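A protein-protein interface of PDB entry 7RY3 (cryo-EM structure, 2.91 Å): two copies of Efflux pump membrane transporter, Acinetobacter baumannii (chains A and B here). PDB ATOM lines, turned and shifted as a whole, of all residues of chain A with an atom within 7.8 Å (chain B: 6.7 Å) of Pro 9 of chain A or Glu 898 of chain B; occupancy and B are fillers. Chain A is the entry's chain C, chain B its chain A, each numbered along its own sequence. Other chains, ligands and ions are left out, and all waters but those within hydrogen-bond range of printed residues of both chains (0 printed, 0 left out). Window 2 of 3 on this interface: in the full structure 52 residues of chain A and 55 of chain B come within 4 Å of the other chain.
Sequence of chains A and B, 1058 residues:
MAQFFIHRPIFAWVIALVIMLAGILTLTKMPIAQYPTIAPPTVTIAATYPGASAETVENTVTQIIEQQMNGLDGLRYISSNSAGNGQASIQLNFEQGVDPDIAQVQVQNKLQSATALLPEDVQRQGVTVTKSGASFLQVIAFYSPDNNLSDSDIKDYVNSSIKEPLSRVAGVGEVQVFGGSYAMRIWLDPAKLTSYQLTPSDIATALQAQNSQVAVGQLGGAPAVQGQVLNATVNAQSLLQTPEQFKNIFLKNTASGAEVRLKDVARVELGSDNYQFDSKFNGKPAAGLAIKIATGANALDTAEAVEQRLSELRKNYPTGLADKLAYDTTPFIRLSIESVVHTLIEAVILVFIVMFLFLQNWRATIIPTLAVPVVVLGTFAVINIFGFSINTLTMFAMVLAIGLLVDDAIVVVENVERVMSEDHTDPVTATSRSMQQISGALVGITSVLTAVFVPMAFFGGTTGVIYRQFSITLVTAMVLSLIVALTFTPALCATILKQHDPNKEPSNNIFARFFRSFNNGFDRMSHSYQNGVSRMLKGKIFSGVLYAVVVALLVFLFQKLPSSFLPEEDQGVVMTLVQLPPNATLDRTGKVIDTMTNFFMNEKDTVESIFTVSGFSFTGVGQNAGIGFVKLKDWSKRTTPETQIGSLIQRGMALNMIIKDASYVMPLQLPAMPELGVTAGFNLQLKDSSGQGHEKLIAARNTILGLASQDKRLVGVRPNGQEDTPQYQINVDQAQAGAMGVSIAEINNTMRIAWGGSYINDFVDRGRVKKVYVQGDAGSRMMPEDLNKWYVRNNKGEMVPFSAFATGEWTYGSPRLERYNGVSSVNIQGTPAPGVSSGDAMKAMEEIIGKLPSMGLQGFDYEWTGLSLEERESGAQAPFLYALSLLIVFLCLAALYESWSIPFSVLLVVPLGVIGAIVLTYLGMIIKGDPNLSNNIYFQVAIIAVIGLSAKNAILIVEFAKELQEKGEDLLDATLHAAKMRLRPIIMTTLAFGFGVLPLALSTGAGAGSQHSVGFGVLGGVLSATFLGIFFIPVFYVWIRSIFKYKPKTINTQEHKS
OE1 of Glu 898 of chain B lies within hydrogen-bond range of N of Ile 10 of chain A. OE2 of Glu 898 of chain B lies within hydrogen-bond range of N of Phe 11 of chain A (3.2 Å).
O of Phe 4 of chain A sits at hydrogen-bond distance from NH1 of Arg 8 of chain A, at 3.2 Å.
Among the printed residues, merely in contact across the chains: Arg 8 of chain A with Glu 898 of chain B, Pro 9 of chain A with Glu 898 of chain B, Ile 10 of chain A with Ala 894 of chain B, Ile 10 of chain A with Ser 899 of chain B, Ile 10 of chain A with Trp 900 of chain B and Phe 11 of chain A with Ala 895 of chain B.
Of chain B, only Glu 898 (3.5 Å) comes within 4 Å of Pro 9 of chain A. Glu 898 of chain B touches four residues of chain A. Printed residues of chain A within 4 Å of Trp 900 of chain B: Ile 10. Of the printed residues of chain B, Phe 11 of chain A touches Ala 895 (3.4 Å) and Glu 898 (3.2 Å). Printed residues of chain A within 4 Å of Ser 899 of chain B: Ile 10. Of the printed residues of chain A, Ala 894 of chain B touches Ile 10. Printed residues of chain B within 4 Å of Arg 8 of chain A: Glu 898. Leu 896 of chain B touches none of the printed residues of chain A. Phe 488 of chain A touches none of the printed residues of chain B. The nearest printed residue of chain B that does not touch Pro 9 of chain A is Trp 900 of chain B (6.8 Å). The nearest residue of chain A that does not touch Glu 898 of chain B is His 7 of chain A (4.8 Å). The nearest printed residue of chain A that does not touch Ala 894 of chain B is Val 14 of chain A (4.01 Å).
Printed residues of chain B that touch a printed residue of chain A: Ala 894, Ala 895, Glu 898, Ser 899 and Trp 900. Along chain B the printed residues that touch a printed residue of chain A span positions 894 to 900. Of the 20 printed residues of chain A, 4 touch a printed residue of chain B. Hydrophobic or aromatic side chains of chain A within 4 Å of the printed part of chain B: Pro 9, Ile 10 and Phe 11. Among the printed residues, 8 pairs touch across the chains.
No position is printed for both chains.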
ATOM      1  N   PHE A   4     -14.177  19.760  -0.339  1.00  0.00           N
ATOM      2  CA  PHE A   4     -15.045  18.916  -1.142  1.00  0.00           C
ATOM      3  C   PHE A   4     -15.293  19.570  -2.472  1.00  0.00           C
ATOM      4  O   PHE A   4     -15.165  18.932  -3.510  1.00  0.00           O
ATOM      5  CB  PHE A   4     -16.390  18.816  -0.435  1.00  0.00           C
ATOM      6  CG  PHE A   4     -17.422  18.005  -1.159  1.00  0.00           C
ATOM      7  CD1 PHE A   4     -17.403  16.628  -1.103  1.00  0.00           C
ATOM      8  CD2 PHE A   4     -18.443  18.625  -1.854  1.00  0.00           C
ATOM      9  CE1 PHE A   4     -18.362  15.883  -1.754  1.00  0.00           C
ATOM     10  CE2 PHE A   4     -19.406  17.888  -2.508  1.00  0.00           C
ATOM     11  CZ  PHE A   4     -19.367  16.514  -2.456  1.00  0.00           C
ATOM     12  N   PHE A   5     -15.622  20.853  -2.450  1.00  0.00           N
ATOM     13  CA  PHE A   5     -15.972  21.574  -3.673  1.00  0.00           C
ATOM     14  C   PHE A   5     -14.830  21.932  -4.603  1.00  0.00           C
ATOM     15  O   PHE A   5     -15.042  22.140  -5.782  1.00  0.00           O
ATOM     16  CB  PHE A   5     -16.887  22.757  -3.345  1.00  0.00           C
ATOM     17  CG  PHE A   5     -18.290  22.353  -3.024  1.00  0.00           C
ATOM     18  CD1 PHE A   5     -19.177  22.035  -4.035  1.00  0.00           C
ATOM     19  CD2 PHE A   5     -18.723  22.289  -1.714  1.00  0.00           C
ATOM     20  CE1 PHE A   5     -20.473  21.659  -3.748  1.00  0.00           C
ATOM     21  CE2 PHE A   5     -20.015  21.909  -1.418  1.00  0.00           C
ATOM     22  CZ  PHE A   5     -20.893  21.597  -2.438  1.00  0.00           C
ATOM     23  N   ILE A   6     -13.625  22.058  -4.066  1.00  0.00           N
ATOM     24  CA  ILE A   6     -12.458  22.355  -4.886  1.00  0.00           C
ATOM     25  C   ILE A   6     -12.215  21.213  -5.847  1.00  0.00           C
ATOM     26  O   ILE A   6     -11.923  21.422  -7.020  1.00  0.00           O
ATOM     27  CB  ILE A   6     -11.224  22.619  -4.016  1.00  0.00           C
ATOM     28  CG1 ILE A   6     -11.194  24.072  -3.561  1.00  0.00           C
ATOM     29  CG2 ILE A   6      -9.935  22.320  -4.759  1.00  0.00           C
ATOM     30  CD1 ILE A   6     -10.252  24.317  -2.404  1.00  0.00           C
ATOM     31  N   HIS A   7     -12.393  20.000  -5.367  1.00  0.00           N
ATOM     32  CA  HIS A   7     -12.184  18.833  -6.189  1.00  0.00           C
ATOM     33  C   HIS A   7     -13.402  18.461  -6.993  1.00  0.00           C
ATOM     34  O   HIS A   7     -13.352  17.557  -7.816  1.00  0.00           O
ATOM     35  CB  HIS A   7     -11.748  17.700  -5.296  1.00  0.00           C
ATOM     36  CG  HIS A   7     -10.372  17.886  -4.747  1.00  0.00           C
ATOM     37  ND1 HIS A   7     -10.135  18.373  -3.482  1.00  0.00           N
ATOM     38  CD2 HIS A   7      -9.158  17.688  -5.309  1.00  0.00           C
ATOM     39  CE1 HIS A   7      -8.832  18.445  -3.278  1.00  0.00           C
ATOM     40  NE2 HIS A   7      -8.217  18.036  -4.372  1.00  0.00           N
ATOM     41  N   ARG A   8     -14.498  19.159  -6.770  1.00  0.00           N
ATOM     42  CA  ARG A   8     -15.714  18.917  -7.524  1.00  0.00           C
ATOM     43  C   ARG A   8     -16.281  20.207  -8.079  1.00  0.00           C
ATOM     44  O   ARG A   8     -17.283  20.696  -7.579  1.00  0.00           O
ATOM     45  CB  ARG A   8     -16.745  18.223  -6.649  1.00  0.00           C
ATOM     46  CG  ARG A   8     -16.499  16.742  -6.481  1.00  0.00           C
ATOM     47  CD  ARG A   8     -17.301  16.191  -5.326  1.00  0.00           C
ATOM     48  NE  ARG A   8     -16.820  14.878  -4.915  1.00  0.00           N
ATOM     49  CZ  ARG A   8     -15.825  14.684  -4.055  1.00  0.00           C
ATOM     50  NH1 ARG A   8     -15.197  15.718  -3.512  1.00  0.00           N
ATOM     51  NH2 ARG A   8     -15.455  13.452  -3.740  1.00  0.00           N
ATOM     52  N   PRO A   9     -15.659  20.747  -9.143  1.00  0.00           N
ATOM     53  CA  PRO A   9     -16.101  22.039  -9.686  1.00  0.00           C
ATOM     54  C   PRO A   9     -17.534  22.104 -10.195  1.00  0.00           C
ATOM     55  O   PRO A   9     -18.211  23.069  -9.896  1.00  0.00           O
ATOM     56  CB  PRO A   9     -15.162  22.246 -10.863  1.00  0.00           C
ATOM     57  CG  PRO A   9     -13.963  21.431 -10.555  1.00  0.00           C
ATOM     58  CD  PRO A   9     -14.489  20.221  -9.861  1.00  0.00           C
ATOM     59  N   ILE A  10     -17.987  21.102 -10.927  1.00  0.00           N
ATOM     60  CA  ILE A  10     -19.353  21.057 -11.476  1.00  0.00           C
ATOM     61  C   ILE A  10     -20.473  21.007 -10.415  1.00  0.00           C
ATOM     62  O   ILE A  10     -21.510  21.616 -10.596  1.00  0.00           O
ATOM     63  CB  ILE A  10     -19.461  19.961 -12.549  1.00  0.00           C
ATOM     64  CG1 ILE A  10     -18.509  20.310 -13.694  1.00  0.00           C
ATOM     65  CG2 ILE A  10     -20.881  19.789 -13.061  1.00  0.00           C
ATOM     66  CD1 ILE A  10     -18.268  19.201 -14.686  1.00  0.00           C
ATOM     67  N   PHE A  11     -20.261  20.326  -9.301  1.00  0.00           N
ATOM     68  CA  PHE A  11     -21.252  20.293  -8.249  1.00  0.00           C
ATOM     69  C   PHE A  11     -21.489  21.725  -7.795  1.00  0.00           C
ATOM     70  O   PHE A  11     -22.623  22.122  -7.577  1.00  0.00           O
ATOM     71  CB  PHE A  11     -20.695  19.467  -7.088  1.00  0.00           C
ATOM     72  CG  PHE A  11     -21.734  18.836  -6.209  1.00  0.00           C
ATOM     73  CD1 PHE A  11     -22.812  19.559  -5.733  1.00  0.00           C
ATOM     74  CD2 PHE A  11     -21.603  17.518  -5.822  1.00  0.00           C
ATOM     75  CE1 PHE A  11     -23.752  18.974  -4.916  1.00  0.00           C
ATOM     76  CE2 PHE A  11     -22.538  16.924  -5.003  1.00  0.00           C
ATOM     77  CZ  PHE A  11     -23.615  17.654  -4.549  1.00  0.00           C
ATOM     78  N   ALA A  12     -20.432  22.505  -7.645  1.00  0.00           N
ATOM     79  CA  ALA A  12     -20.545  23.905  -7.256  1.00  0.00           C
ATOM     80  C   ALA A  12     -21.243  24.780  -8.276  1.00  0.00           C
ATOM     81  O   ALA A  12     -22.006  25.666  -7.908  1.00  0.00           O
ATOM     82  CB  ALA A  12     -19.164  24.446  -6.964  1.00  0.00           C
ATOM     83  N   TRP A  13     -20.958  24.566  -9.550  1.00  0.00           N
ATOM     84  CA  TRP A  13     -21.628  25.303 -10.608  1.00  0.00           C
ATOM     85  C   TRP A  13     -23.100  24.974 -10.631  1.00  0.00           C
ATOM     86  O   TRP A  13     -23.925  25.815 -10.928  1.00  0.00           O
ATOM     87  CB  TRP A  13     -20.991  25.053 -11.970  1.00  0.00           C
ATOM     88  CG  TRP A  13     -19.911  25.983 -12.348  1.00  0.00           C
ATOM     89  CD1 TRP A  13     -18.573  25.766 -12.248  1.00  0.00           C
ATOM     90  CD2 TRP A  13     -20.068  27.280 -12.920  1.00  0.00           C
ATOM     91  NE1 TRP A  13     -17.883  26.854 -12.713  1.00  0.00           N
ATOM     92  CE2 TRP A  13     -18.781  27.799 -13.131  1.00  0.00           C
ATOM     93  CE3 TRP A  13     -21.175  28.059 -13.264  1.00  0.00           C
ATOM     94  CZ2 TRP A  13     -18.570  29.057 -13.671  1.00  0.00           C
ATOM     95  CZ3 TRP A  13     -20.962  29.301 -13.802  1.00  0.00           C
ATOM     96  CH2 TRP A  13     -19.671  29.791 -13.998  1.00  0.00           C
ATOM     97  N   VAL A  14     -23.431  23.728 -10.360  1.00  0.00           N
ATOM     98  CA  VAL A  14     -24.823  23.334 -10.307  1.00  0.00           C
ATOM     99  C   VAL A  14     -25.568  24.018  -9.183  1.00  0.00           C
ATOM    100  O   VAL A  14     -26.666  24.507  -9.384  1.00  0.00           O
ATOM    101  CB  VAL A  14     -24.991  21.797 -10.282  1.00  0.00           C
ATOM    102  CG1 VAL A  14     -26.412  21.396  -9.921  1.00  0.00           C
ATOM    103  CG2 VAL A  14     -24.593  21.203 -11.623  1.00  0.00           C
ATOM    104  N   ILE A  15     -24.952  24.116  -8.016  1.00  0.00           N
ATOM    105  CA  ILE A  15     -25.603  24.801  -6.902  1.00  0.00           C
ATOM    106  C   ILE A  15     -25.805  26.252  -7.249  1.00  0.00           C
ATOM    107  O   ILE A  15     -26.875  26.801  -7.032  1.00  0.00           O
ATOM    108  CB  ILE A  15     -24.802  24.705  -5.598  1.00  0.00           C
ATOM    109  CG1 ILE A  15     -24.551  23.250  -5.216  1.00  0.00           C
ATOM    110  CG2 ILE A  15     -25.524  25.416  -4.468  1.00  0.00           C
ATOM    111  CD1 ILE A  15     -25.812  22.433  -5.053  1.00  0.00           C
ATOM    112  N   VAL A 428      -4.871  24.113  -7.389  1.00  0.00           N
ATOM    113  CA  VAL A 428      -5.618  23.249  -6.485  1.00  0.00           C
ATOM    114  C   VAL A 428      -4.888  23.116  -5.159  1.00  0.00           C
ATOM    115  O   VAL A 428      -5.514  23.037  -4.115  1.00  0.00           O
ATOM    116  CB  VAL A 428      -5.907  21.893  -7.135  1.00  0.00           C
ATOM    117  CG1 VAL A 428      -6.815  21.051  -6.260  1.00  0.00           C
ATOM    118  CG2 VAL A 428      -6.532  22.103  -8.502  1.00  0.00           C
ATOM    119  N   THR A 487     -18.348  27.155  -1.337  1.00  0.00           N
ATOM    120  CA  THR A 487     -18.710  26.300  -2.457  1.00  0.00           C
ATOM    121  C   THR A 487     -18.254  26.837  -3.788  1.00  0.00           C
ATOM    122  O   THR A 487     -17.300  26.316  -4.356  1.00  0.00           O
ATOM    123  CB  THR A 487     -20.222  26.027  -2.511  1.00  0.00           C
ATOM    124  OG1 THR A 487     -20.938  27.251  -2.703  1.00  0.00           O
ATOM    125  CG2 THR A 487     -20.705  25.384  -1.231  1.00  0.00           C
ATOM    126  N   PHE A 488     -18.910  27.861  -4.304  1.00  0.00           N
ATOM    127  CA  PHE A 488     -18.602  28.386  -5.625  1.00  0.00           C
ATOM    128  C   PHE A 488     -17.248  29.034  -5.778  1.00  0.00           C
ATOM    129  O   PHE A 488     -16.526  28.753  -6.731  1.00  0.00           O
ATOM    130  CB  PHE A 488     -19.694  29.395  -5.981  1.00  0.00           C
ATOM    131  CG  PHE A 488     -19.823  29.684  -7.447  1.00  0.00           C
ATOM    132  CD1 PHE A 488     -19.614  28.698  -8.388  1.00  0.00           C
ATOM    133  CD2 PHE A 488     -20.201  30.945  -7.876  1.00  0.00           C
ATOM    134  CE1 PHE A 488     -19.748  28.969  -9.731  1.00  0.00           C
ATOM    135  CE2 PHE A 488     -20.340  31.222  -9.220  1.00  0.00           C
ATOM    136  CZ  PHE A 488     -20.113  30.231 -10.148  1.00  0.00           C
ATOM    137  N   PRO A 490     -14.114  28.867  -4.103  1.00  0.00           N
ATOM    138  CA  PRO A 490     -12.882  28.085  -4.138  1.00  0.00           C
ATOM    139  C   PRO A 490     -12.737  27.259  -5.405  1.00  0.00           C
ATOM    140  O   PRO A 490     -11.630  27.104  -5.878  1.00  0.00           O
ATOM    141  CB  PRO A 490     -13.001  27.208  -2.906  1.00  0.00           C
ATOM    142  CG  PRO A 490     -13.920  27.932  -2.003  1.00  0.00           C
ATOM    143  CD  PRO A 490     -14.926  28.509  -2.929  1.00  0.00           C
ATOM    144  N   ALA A 491     -13.825  26.729  -5.938  1.00  0.00           N
ATOM    145  CA  ALA A 491     -13.771  25.952  -7.152  1.00  0.00           C
ATOM    146  C   ALA A 491     -13.428  26.841  -8.321  1.00  0.00           C
ATOM    147  O   ALA A 491     -12.684  26.445  -9.194  1.00  0.00           O
ATOM    148  CB  ALA A 491     -15.085  25.247  -7.383  1.00  0.00           C
ATOM    149  N   LEU A 492     -13.969  28.051  -8.352  1.00  0.00           N
ATOM    150  CA  LEU A 492     -13.610  29.002  -9.396  1.00  0.00           C
ATOM    151  C   LEU A 492     -12.165  29.344  -9.259  1.00  0.00           C
ATOM    152  O   LEU A 492     -11.447  29.431 -10.232  1.00  0.00           O
ATOM    153  CB  LEU A 492     -14.447  30.272  -9.276  1.00  0.00           C
ATOM    154  CG  LEU A 492     -15.953  30.223  -9.490  1.00  0.00           C
ATOM    155  CD1 LEU A 492     -16.594  31.559  -9.180  1.00  0.00           C
ATOM    156  CD2 LEU A 492     -16.260  29.771 -10.906  1.00  0.00           C
ATOM    157  N   ALA A 494      -9.822  27.465  -7.930  1.00  0.00           N
ATOM    158  CA  ALA A 494      -9.027  26.337  -8.406  1.00  0.00           C
ATOM    159  C   ALA A 494      -9.001  26.216  -9.911  1.00  0.00           C
ATOM    160  O   ALA A 494      -7.937  26.040 -10.494  1.00  0.00           O
ATOM    161  CB  ALA A 494      -9.525  25.051  -7.800  1.00  0.00           C
ATOM    162  N   THR A 495     -10.158  26.305 -10.551  1.00  0.00           N
ATOM    163  CA  THR A 495     -10.230  26.255 -12.005  1.00  0.00           C
ATOM    164  C   THR A 495      -9.749  27.436 -12.862  1.00  0.00           C
ATOM    165  O   THR A 495      -8.971  27.241 -13.784  1.00  0.00           O
ATOM    166  CB  THR A 495     -11.661  25.929 -12.434  1.00  0.00           C
ATOM    167  OG1 THR A 495     -12.567  26.893 -11.890  1.00  0.00           O
ATOM    168  CG2 THR A 495     -12.045  24.546 -11.949  1.00  0.00           C
ATOM    169  N   LEU B 893     -27.673  14.890 -12.333  1.00  0.00           N
ATOM    170  CA  LEU B 893     -26.724  13.963 -12.900  1.00  0.00           C
ATOM    171  C   LEU B 893     -25.336  14.558 -12.966  1.00  0.00           C
ATOM    172  O   LEU B 893     -24.370  13.873 -12.695  1.00  0.00           O
ATOM    173  CB  LEU B 893     -27.196  13.495 -14.270  1.00  0.00           C
ATOM    174  CG  LEU B 893     -28.286  12.436 -14.289  1.00  0.00           C
ATOM    175  CD1 LEU B 893     -28.585  12.065 -15.728  1.00  0.00           C
ATOM    176  CD2 LEU B 893     -27.821  11.228 -13.505  1.00  0.00           C
ATOM    177  N   ALA B 894     -25.232  15.821 -13.348  1.00  0.00           N
ATOM    178  CA  ALA B 894     -23.940  16.494 -13.386  1.00  0.00           C
ATOM    179  C   ALA B 894     -23.291  16.503 -12.024  1.00  0.00           C
ATOM    180  O   ALA B 894     -22.145  16.130 -11.886  1.00  0.00           O
ATOM    181  CB  ALA B 894     -24.122  17.909 -13.861  1.00  0.00           C
ATOM    182  N   ALA B 895     -24.024  16.915 -11.000  1.00  0.00           N
ATOM    183  CA  ALA B 895     -23.458  17.014  -9.688  1.00  0.00           C
ATOM    184  C   ALA B 895     -22.993  15.678  -9.221  1.00  0.00           C
ATOM    185  O   ALA B 895     -21.931  15.570  -8.620  1.00  0.00           O
ATOM    186  CB  ALA B 895     -24.503  17.539  -8.753  1.00  0.00           C
ATOM    187  N   LEU B 896     -23.790  14.657  -9.450  1.00  0.00           N
ATOM    188  CA  LEU B 896     -23.400  13.315  -9.093  1.00  0.00           C
ATOM    189  C   LEU B 896     -22.226  12.777  -9.900  1.00  0.00           C
ATOM    190  O   LEU B 896     -21.310  12.194  -9.350  1.00  0.00           O
ATOM    191  CB  LEU B 896     -24.621  12.410  -9.238  1.00  0.00           C
ATOM    192  CG  LEU B 896     -24.561  11.006  -8.642  1.00  0.00           C
ATOM    193  CD1 LEU B 896     -24.231  11.072  -7.160  1.00  0.00           C
ATOM    194  CD2 LEU B 896     -25.886  10.296  -8.864  1.00  0.00           C
ATOM    195  N   TYR B 897     -22.237  12.991 -11.203  1.00  0.00           N
ATOM    196  CA  TYR B 897     -21.186  12.450 -12.058  1.00  0.00           C
ATOM    197  C   TYR B 897     -20.115  13.390 -12.567  1.00  0.00           C
ATOM    198  O   TYR B 897     -19.334  12.987 -13.418  1.00  0.00           O
ATOM    199  CB  TYR B 897     -21.787  11.652 -13.200  1.00  0.00           C
ATOM    200  CG  TYR B 897     -22.597  10.491 -12.688  1.00  0.00           C
ATOM    201  CD1 TYR B 897     -21.985   9.447 -12.015  1.00  0.00           C
ATOM    202  CD2 TYR B 897     -23.970  10.452 -12.843  1.00  0.00           C
ATOM    203  CE1 TYR B 897     -22.717   8.390 -11.522  1.00  0.00           C
ATOM    204  CE2 TYR B 897     -24.710   9.396 -12.355  1.00  0.00           C
ATOM    205  CZ  TYR B 897     -24.077   8.370 -11.695  1.00  0.00           C
ATOM    206  OH  TYR B 897     -24.805   7.317 -11.205  1.00  0.00           O
ATOM    207  N   GLU B 898     -20.098  14.646 -12.119  1.00  0.00           N
ATOM    208  CA  GLU B 898     -19.035  15.591 -12.461  1.00  0.00           C
ATOM    209  C   GLU B 898     -18.760  15.725 -13.917  1.00  0.00           C
ATOM    210  O   GLU B 898     -17.611  15.742 -14.328  1.00  0.00           O
ATOM    211  CB  GLU B 898     -17.753  15.285 -11.711  1.00  0.00           C
ATOM    212  CG  GLU B 898     -17.804  15.631 -10.236  1.00  0.00           C
ATOM    213  CD  GLU B 898     -18.095  17.097 -10.001  1.00  0.00           C
ATOM    214  OE1 GLU B 898     -17.314  17.946 -10.482  1.00  0.00           O
ATOM    215  OE2 GLU B 898     -19.103  17.394  -9.323  1.00  0.00           O
ATOM    216  N   SER B 899     -19.806  15.763 -14.716  1.00  0.00           N
ATOM    217  CA  SER B 899     -19.635  15.932 -16.129  1.00  0.00           C
ATOM    218  C   SER B 899     -20.741  16.740 -16.686  1.00  0.00           C
ATOM    219  O   SER B 899     -21.728  16.985 -16.023  1.00  0.00           O
ATOM    220  CB  SER B 899     -19.608  14.568 -16.834  1.00  0.00           C
ATOM    221  OG  SER B 899     -19.478  14.702 -18.237  1.00  0.00           O
ATOM    222  N   TRP B 900     -20.579  17.178 -17.909  1.00  0.00           N
ATOM    223  CA  TRP B 900     -21.650  17.849 -18.585  1.00  0.00           C
ATOM    224  C   TRP B 900     -22.015  16.953 -19.735  1.00  0.00           C
ATOM    225  O   TRP B 900     -23.174  16.852 -20.110  1.00  0.00           O
ATOM    226  CB  TRP B 900     -21.166  19.195 -19.098  1.00  0.00           C
ATOM    227  CG  TRP B 900     -20.977  20.235 -18.042  1.00  0.00           C
ATOM    228  CD1 TRP B 900     -19.807  20.830 -17.689  1.00  0.00           C
ATOM    229  CD2 TRP B 900     -21.988  20.808 -17.203  1.00  0.00           C
ATOM    230  NE1 TRP B 900     -20.022  21.737 -16.686  1.00  0.00           N
ATOM    231  CE2 TRP B 900     -21.353  21.741 -16.367  1.00  0.00           C
ATOM    232  CE3 TRP B 900     -23.365  20.621 -17.078  1.00  0.00           C
ATOM    233  CZ2 TRP B 900     -22.046  22.485 -15.421  1.00  0.00           C
ATOM    234  CZ3 TRP B 900     -24.048  21.360 -16.137  1.00  0.00           C
ATOM    235  CH2 TRP B 900     -23.390  22.280 -15.323  1.00  0.00           C
ATOM    236  N   PRO B 903     -24.495  13.826 -18.692  1.00  0.00           N
ATOM    237  CA  PRO B 903     -25.920  14.121 -18.592  1.00  0.00           C
ATOM    238  C   PRO B 903     -26.629  14.277 -19.944  1.00  0.00           C
ATOM    239  O   PRO B 903     -27.770  13.862 -20.057  1.00  0.00           O
ATOM    240  CB  PRO B 903     -25.930  15.417 -17.798  1.00  0.00           C
ATOM    241  CG  PRO B 903     -24.790  15.283 -16.881  1.00  0.00           C
ATOM    242  CD  PRO B 903     -23.741  14.533 -17.637  1.00  0.00           C
ATOM    243  N   LYS B 962     -17.896   4.525 -17.243  1.00  0.00           N
ATOM    244  CA  LYS B 962     -16.984   5.611 -16.949  1.00  0.00           C
ATOM    245  C   LYS B 962     -15.969   5.120 -15.966  1.00  0.00           C
ATOM    246  O   LYS B 962     -14.815   5.484 -16.044  1.00  0.00           O
ATOM    247  CB  LYS B 962     -17.791   6.729 -16.319  1.00  0.00           C
ATOM    248  CG  LYS B 962     -16.994   7.893 -15.768  1.00  0.00           C
ATOM    249  CD  LYS B 962     -17.911   8.868 -15.055  1.00  0.00           C
ATOM    250  CE  LYS B 962     -17.142  10.055 -14.511  1.00  0.00           C
ATOM    251  NZ  LYS B 962     -16.333  10.722 -15.566  1.00  0.00           N
